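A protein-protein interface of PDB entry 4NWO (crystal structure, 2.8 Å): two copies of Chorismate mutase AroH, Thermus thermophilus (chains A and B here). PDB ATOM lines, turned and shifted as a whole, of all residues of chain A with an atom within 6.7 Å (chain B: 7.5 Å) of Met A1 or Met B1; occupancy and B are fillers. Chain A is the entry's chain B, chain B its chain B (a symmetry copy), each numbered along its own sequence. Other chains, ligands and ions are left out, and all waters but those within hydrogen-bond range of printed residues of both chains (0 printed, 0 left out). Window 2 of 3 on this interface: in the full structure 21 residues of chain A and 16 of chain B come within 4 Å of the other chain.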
ATOM      1  N   MET A   1       1.796  18.359  19.661  1.00  0.00           N
ATOM      2  CA  MET A   1       1.638  17.956  18.271  1.00  0.00           C
ATOM      3  C   MET A   1       0.545  18.776  17.588  1.00  0.00           C
ATOM      4  O   MET A   1      -0.639  18.454  17.679  1.00  0.00           O
ATOM      5  CB  MET A   1       1.326  16.460  18.181  1.00  0.00           C
ATOM      6  CG  MET A   1       1.123  15.941  16.767  1.00  0.00           C
ATOM      7  SD  MET A   1       2.484  16.339  15.651  1.00  0.00           S
ATOM      8  CE  MET A   1       1.871  15.653  14.114  1.00  0.00           C
ATOM      9  N   VAL A   2       0.957  19.848  16.920  1.00  0.00           N
ATOM     10  CA  VAL A   2       0.037  20.884  16.465  1.00  0.00           C
ATOM     11  C   VAL A   2       0.279  21.147  14.982  1.00  0.00           C
ATOM     12  O   VAL A   2       1.411  21.084  14.508  1.00  0.00           O
ATOM     13  CB  VAL A   2       0.194  22.189  17.287  1.00  0.00           C
ATOM     14  CG1 VAL A   2      -0.700  23.300  16.744  1.00  0.00           C
ATOM     15  CG2 VAL A   2      -0.120  21.928  18.747  1.00  0.00           C
ATOM     16  N   ARG A   3      -0.798  21.413  14.250  1.00  0.00           N
ATOM     17  CA  ARG A   3      -0.704  21.876  12.872  1.00  0.00           C
ATOM     18  C   ARG A   3      -1.432  23.207  12.740  1.00  0.00           C
ATOM     19  O   ARG A   3      -2.579  23.338  13.167  1.00  0.00           O
ATOM     20  CB  ARG A   3      -1.305  20.850  11.909  1.00  0.00           C
ATOM     21  CG  ARG A   3      -0.538  19.541  11.799  1.00  0.00           C
ATOM     22  CD  ARG A   3       0.820  19.706  11.136  1.00  0.00           C
ATOM     23  NE  ARG A   3       1.512  18.423  11.034  1.00  0.00           N
ATOM     24  CZ  ARG A   3       2.827  18.285  10.924  1.00  0.00           C
ATOM     25  NH1 ARG A   3       3.610  19.355  10.887  1.00  0.00           N
ATOM     26  NH2 ARG A   3       3.365  17.074  10.883  1.00  0.00           N
ATOM     27  N   GLU A  40     -13.191  21.814  20.419  1.00  0.00           N
ATOM     28  CA  GLU A  40     -12.227  21.339  21.408  1.00  0.00           C
ATOM     29  C   GLU A  40     -10.879  20.934  20.805  1.00  0.00           C
ATOM     30  O   GLU A  40      -9.874  20.844  21.510  1.00  0.00           O
ATOM     31  CB  GLU A  40     -12.818  20.157  22.184  1.00  0.00           C
ATOM     32  N   ALA A  43      -6.397  24.558  19.612  1.00  0.00           N
ATOM     33  CA  ALA A  43      -5.579  25.173  20.652  1.00  0.00           C
ATOM     34  C   ALA A  43      -5.894  26.661  20.758  1.00  0.00           C
ATOM     35  O   ALA A  43      -6.075  27.189  21.856  1.00  0.00           O
ATOM     36  CB  ALA A  43      -4.101  24.962  20.365  1.00  0.00           C
ATOM     37  N   TRP A  94      -4.235  23.732  15.409  1.00  0.00           N
ATOM     38  CA  TRP A  94      -5.042  22.525  15.489  1.00  0.00           C
ATOM     39  C   TRP A  94      -4.299  21.358  16.136  1.00  0.00           C
ATOM     40  O   TRP A  94      -3.239  20.952  15.660  1.00  0.00           O
ATOM     41  CB  TRP A  94      -5.513  22.157  14.077  1.00  0.00           C
ATOM     42  CG  TRP A  94      -6.363  20.936  13.968  1.00  0.00           C
ATOM     43  CD1 TRP A  94      -7.142  20.381  14.941  1.00  0.00           C
ATOM     44  CD2 TRP A  94      -6.545  20.130  12.798  1.00  0.00           C
ATOM     45  NE1 TRP A  94      -7.784  19.267  14.453  1.00  0.00           N
ATOM     46  CE2 TRP A  94      -7.436  19.093  13.139  1.00  0.00           C
ATOM     47  CE3 TRP A  94      -6.035  20.180  11.497  1.00  0.00           C
ATOM     48  CZ2 TRP A  94      -7.828  18.115  12.226  1.00  0.00           C
ATOM     49  CZ3 TRP A  94      -6.426  19.209  10.591  1.00  0.00           C
ATOM     50  CH2 TRP A  94      -7.314  18.190  10.961  1.00  0.00           C
ATOM     51  N   ASN A  95      -4.861  20.824  17.218  1.00  0.00           N
ATOM     52  CA  ASN A  95      -4.315  19.628  17.855  1.00  0.00           C
ATOM     53  C   ASN A  95      -4.683  18.383  17.053  1.00  0.00           C
ATOM     54  O   ASN A  95      -5.822  17.918  17.092  1.00  0.00           O
ATOM     55  CB  ASN A  95      -4.821  19.501  19.295  1.00  0.00           C
ATOM     56  CG  ASN A  95      -4.228  20.550  20.217  1.00  0.00           C
ATOM     57  OD1 ASN A  95      -3.016  20.752  20.250  1.00  0.00           O
ATOM     58  ND2 ASN A  95      -5.087  21.226  20.973  1.00  0.00           N
ATOM     59  N   THR A  96      -3.702  17.852  16.330  1.00  0.00           N
ATOM     60  CA  THR A  96      -3.920  16.766  15.381  1.00  0.00           C
ATOM     61  C   THR A  96      -2.602  16.067  15.063  1.00  0.00           C
ATOM     62  O   THR A  96      -1.531  16.646  15.232  1.00  0.00           O
ATOM     63  CB  THR A  96      -4.561  17.272  14.074  1.00  0.00           C
ATOM     64  OG1 THR A  96      -4.914  16.156  13.248  1.00  0.00           O
ATOM     65  CG2 THR A  96      -3.597  18.174  13.320  1.00  0.00           C
ATOM     66  N   ASP A  97      -2.683  14.823  14.603  1.00  0.00           N
ATOM     67  CA  ASP A  97      -1.511  14.143  14.061  1.00  0.00           C
ATOM     68  C   ASP A  97      -1.509  14.097  12.535  1.00  0.00           C
ATOM     69  O   ASP A  97      -0.722  13.364  11.932  1.00  0.00           O
ATOM     70  CB  ASP A  97      -1.422  12.720  14.619  1.00  0.00           C
ATOM     71  N   THR A  98      -2.404  14.867  11.920  1.00  0.00           N
ATOM     72  CA  THR A  98      -2.464  15.006  10.465  1.00  0.00           C
ATOM     73  C   THR A  98      -1.104  15.396   9.887  1.00  0.00           C
ATOM     74  O   THR A  98      -0.459  16.315  10.392  1.00  0.00           O
ATOM     75  CB  THR A  98      -3.508  16.063  10.050  1.00  0.00           C
ATOM     76  OG1 THR A  98      -4.795  15.693  10.558  1.00  0.00           O
ATOM     77  CG2 THR A  98      -3.580  16.186   8.537  1.00  0.00           C
ATOM     78  N   PRO A  99      -0.654  14.692   8.834  1.00  0.00           N
ATOM     79  CA  PRO A  99       0.593  15.102   8.179  1.00  0.00           C
ATOM     80  C   PRO A  99       0.512  16.521   7.622  1.00  0.00           C
ATOM     81  O   PRO A  99      -0.577  16.971   7.264  1.00  0.00           O
ATOM     82  CB  PRO A  99       0.750  14.083   7.047  1.00  0.00           C
ATOM     83  CG  PRO A  99      -0.029  12.893   7.493  1.00  0.00           C
ATOM     84  CD  PRO A  99      -1.182  13.430   8.291  1.00  0.00           C
ATOM     85  N   MET B   1      -0.217  18.815  21.751  1.00  0.00           N
ATOM     86  CA  MET B   1      -1.388  18.965  22.602  1.00  0.00           C
ATOM     87  C   MET B   1      -1.306  20.255  23.417  1.00  0.00           C
ATOM     88  O   MET B   1      -0.690  20.295  24.481  1.00  0.00           O
ATOM     89  CB  MET B   1      -1.535  17.753  23.525  1.00  0.00           C
ATOM     90  CG  MET B   1      -2.722  17.820  24.472  1.00  0.00           C
ATOM     91  SD  MET B   1      -4.291  18.135  23.640  1.00  0.00           S
ATOM     92  CE  MET B   1      -5.405  18.217  25.040  1.00  0.00           C
ATOM     93  N   VAL B   2      -1.921  21.310  22.893  1.00  0.00           N
ATOM     94  CA  VAL B   2      -1.698  22.665  23.384  1.00  0.00           C
ATOM     95  C   VAL B   2      -3.047  23.319  23.667  1.00  0.00           C
ATOM     96  O   VAL B   2      -4.023  23.079  22.960  1.00  0.00           O
ATOM     97  CB  VAL B   2      -0.878  23.511  22.378  1.00  0.00           C
ATOM     98  CG1 VAL B   2      -0.731  24.953  22.851  1.00  0.00           C
ATOM     99  CG2 VAL B   2       0.488  22.887  22.163  1.00  0.00           C
ATOM    100  N   ARG B   3      -3.100  24.126  24.722  1.00  0.00           N
ATOM    101  CA  ARG B   3      -4.255  24.968  24.997  1.00  0.00           C
ATOM    102  C   ARG B   3      -3.807  26.422  25.079  1.00  0.00           C
ATOM    103  O   ARG B   3      -2.853  26.743  25.788  1.00  0.00           O
ATOM    104  CB  ARG B   3      -4.935  24.554  26.303  1.00  0.00           C
ATOM    105  CG  ARG B   3      -5.607  23.189  26.277  1.00  0.00           C
ATOM    106  CD  ARG B   3      -6.822  23.146  25.365  1.00  0.00           C
ATOM    107  NE  ARG B   3      -7.445  21.825  25.385  1.00  0.00           N
ATOM    108  CZ  ARG B   3      -8.212  21.340  24.416  1.00  0.00           C
ATOM    109  NH1 ARG B   3      -8.471  22.072  23.341  1.00  0.00           N
ATOM    110  NH2 ARG B   3      -8.696  20.109  24.507  1.00  0.00           N
ATOM    111  N   TRP B  94      -0.055  26.852  26.078  1.00  0.00           N
ATOM    112  CA  TRP B  94       0.232  25.990  27.214  1.00  0.00           C
ATOM    113  C   TRP B  94       0.241  24.508  26.845  1.00  0.00           C
ATOM    114  O   TRP B  94      -0.752  23.983  26.344  1.00  0.00           O
ATOM    115  CB  TRP B  94      -0.798  26.273  28.313  1.00  0.00           C
ATOM    116  CG  TRP B  94      -0.653  25.475  29.566  1.00  0.00           C
ATOM    117  CD1 TRP B  94       0.482  24.891  30.048  1.00  0.00           C
ATOM    118  CD2 TRP B  94      -1.685  25.199  30.521  1.00  0.00           C
ATOM    119  NE1 TRP B  94       0.215  24.252  31.237  1.00  0.00           N
ATOM    120  CE2 TRP B  94      -1.107  24.428  31.550  1.00  0.00           C
ATOM    121  CE3 TRP B  94      -3.043  25.522  30.602  1.00  0.00           C
ATOM    122  CZ2 TRP B  94      -1.841  23.976  32.645  1.00  0.00           C
ATOM    123  CZ3 TRP B  94      -3.769  25.073  31.691  1.00  0.00           C
ATOM    124  CH2 TRP B  94      -3.166  24.308  32.698  1.00  0.00           C
ATOM    125  N   ASN B  95       1.365  23.841  27.098  1.00  0.00           N
ATOM    126  CA  ASN B  95       1.460  22.396  26.907  1.00  0.00           C
ATOM    127  C   ASN B  95       0.769  21.662  28.052  1.00  0.00           C
ATOM    128  O   ASN B  95       1.297  21.577  29.161  1.00  0.00           O
ATOM    129  CB  ASN B  95       2.923  21.958  26.799  1.00  0.00           C
ATOM    130  CG  ASN B  95       3.575  22.409  25.506  1.00  0.00           C
ATOM    131  OD1 ASN B  95       3.033  22.213  24.421  1.00  0.00           O
ATOM    132  ND2 ASN B  95       4.749  23.022  25.619  1.00  0.00           N
ATOM    133  N   THR B  96      -0.416  21.131  27.765  1.00  0.00           N
ATOM    134  CA  THR B  96      -1.282  20.542  28.779  1.00  0.00           C
ATOM    135  C   THR B  96      -2.313  19.624  28.130  1.00  0.00           C
ATOM    136  O   THR B  96      -2.613  19.763  26.946  1.00  0.00           O
ATOM    137  CB  THR B  96      -2.006  21.622  29.607  1.00  0.00           C
ATOM    138  OG1 THR B  96      -2.705  21.006  30.695  1.00  0.00           O
ATOM    139  CG2 THR B  96      -2.994  22.387  28.741  1.00  0.00           C
ATOM    140  N   ASP B  97      -2.853  18.690  28.905  1.00  0.00           N
ATOM    141  CA  ASP B  97      -4.000  17.909  28.454  1.00  0.00           C
ATOM    142  C   ASP B  97      -5.314  18.374  29.078  1.00  0.00           C
ATOM    143  O   ASP B  97      -6.329  17.681  28.987  1.00  0.00           O
ATOM    144  CB  ASP B  97      -3.781  16.425  28.762  1.00  0.00           C
ATOM    145  N   THR B  98      -5.280  19.536  29.726  1.00  0.00           N
ATOM    146  CA  THR B  98      -6.474  20.162  30.294  1.00  0.00           C
ATOM    147  C   THR B  98      -7.584  20.291  29.252  1.00  0.00           C
ATOM    148  O   THR B  98      -7.333  20.750  28.137  1.00  0.00           O
ATOM    149  CB  THR B  98      -6.152  21.559  30.862  1.00  0.00           C
ATOM    150  OG1 THR B  98      -5.135  21.449  31.865  1.00  0.00           O
ATOM    151  CG2 THR B  98      -7.392  22.195  31.470  1.00  0.00           C
ATOM    152  N   PRO B  99      -8.813  19.877  29.602  1.00  0.00           N
ATOM    153  CA  PRO B  99      -9.931  20.083  28.674  1.00  0.00           C
ATOM    154  C   PRO B  99     -10.153  21.561  28.361  1.00  0.00           C
ATOM    155  O   PRO B  99      -9.852  22.411  29.199  1.00  0.00           O
ATOM    156  CB  PRO B  99     -11.129  19.501  29.428  1.00  0.00           C
ATOM    157  CG  PRO B  99     -10.540  18.526  30.388  1.00  0.00           C
ATOM    158  CD  PRO B  99      -9.206  19.089  30.782  1.00  0.00           C
ATOM    159  N   GLN B 100     -10.660  21.852  27.165  1.00  0.00           N
ATOM    160  CA  GLN B 100     -10.889  23.229  26.733  1.00  0.00           C
ATOM    161  C   GLN B 100     -11.768  24.020  27.702  1.00  0.00           C
ATOM    162  O   GLN B 100     -11.528  25.202  27.952  1.00  0.00           O
ATOM    163  CB  GLN B 100     -11.514  23.236  25.334  1.00  0.00           C
ATOM    164  CG  GLN B 100     -11.608  24.611  24.698  1.00  0.00           C
ATOM    165  CD  GLN B 100     -12.045  24.554  23.248  1.00  0.00           C
ATOM    166  OE1 GLN B 100     -13.210  24.298  22.947  1.00  0.00           O
ATOM    167  NE2 GLN B 100     -11.105  24.796  22.337  1.00  0.00           N
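The backbone carbonyl oxygen of Glu A40 lies within hydrogen-bond range of the guanidinium group of Arg B3 (2.6 Å). The backbone NH (N) of Val B2 is in hydrogen-bond range of the side-chain amide oxygen (OD1) of Asn A95, at 2.9 Å. N of Met B1 sits close to N of Met A1, 2.9 Å away.
The backbone carbonyl oxygen (O) of Met A1 lies within hydrogen-bond range of the backbone NH (N) of Thr A96, 3.4 Å away. The backbone carbonyl oxygen (O) of Met B1 sits at hydrogen-bond distance from the backbone NH (N) of Thr B96, 3.4 Å away. The backbone carbonyl oxygen (O) of Arg B3 is in hydrogen-bond range of the backbone NH (N) of Trp B94 (2.8 Å). The backbone carbonyl oxygen (O) of Thr B98 sits at hydrogen-bond distance from the guanidinium group (NE) of Arg B3 (3.0 Å).
Among the printed residues, pairs that only touch across the chains: Val A2 with Val B2 (3.6 Å), Glu A40 with Gln B100 (3.5 Å), Ala A43 with Val B2 (3.2 Å) and Asn A95 with Met B1 (3.4 Å).
Met A1 touches just one residue of chain B: Met B1. Printed residues of chain B within 4 Å of Val A2: Val B2 (3.6 Å). Of the printed residues of chain B, Glu A40 touches Arg B3 and Gln B100. Of the printed residues of chain B, Ala A43 touches Val B2 (3.2 Å). Asp A97 touches none of the printed residues of chain B. Of the printed residues of chain A, Met B1 touches Met A1 (2.9 Å) and Asn A95 (3.4 Å). Printed residues of chain A within 4 Å of Val B2: Val A2, Ala A43 and Asn A95. Asn B95 touches none of the printed residues of chain A. The nearest printed residue of chain B that does not touch Asn A95 is Arg B3 (4.2 Å).
Hydrophobic or aromatic side chains of chain B within 4 Å of the printed part of chain A: Val B2. Of the 11 printed residues of chain A, 5 touch a printed residue of chain B. Printed residues of chain A that touch a printed residue of chain B: Met A1, Val A2, Glu A40, Ala A43 and Asn A95. Hydrophobic or aromatic side chains of chain A within 4 Å of the printed part of chain B: Val A2 and Ala A43. Among the printed residues, 7 pairs touch across the chains. Among the printed residues, no Asp or Glu carboxylate lies within 4 Å of a Lys or Arg side-chain nitrogen of the other chain.
Met A1 touches its own counterpart, Met B1. Val A2 touches its own counterpart, Val B2. Asn A95 touches Met B1, but with the chains exchanged Met A1 does not touch Asn B95 (6.2 Å). Asn A95 touches Val B2, but with the chains exchanged Val A2 does not touch Asn B95 (6.5 Å).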
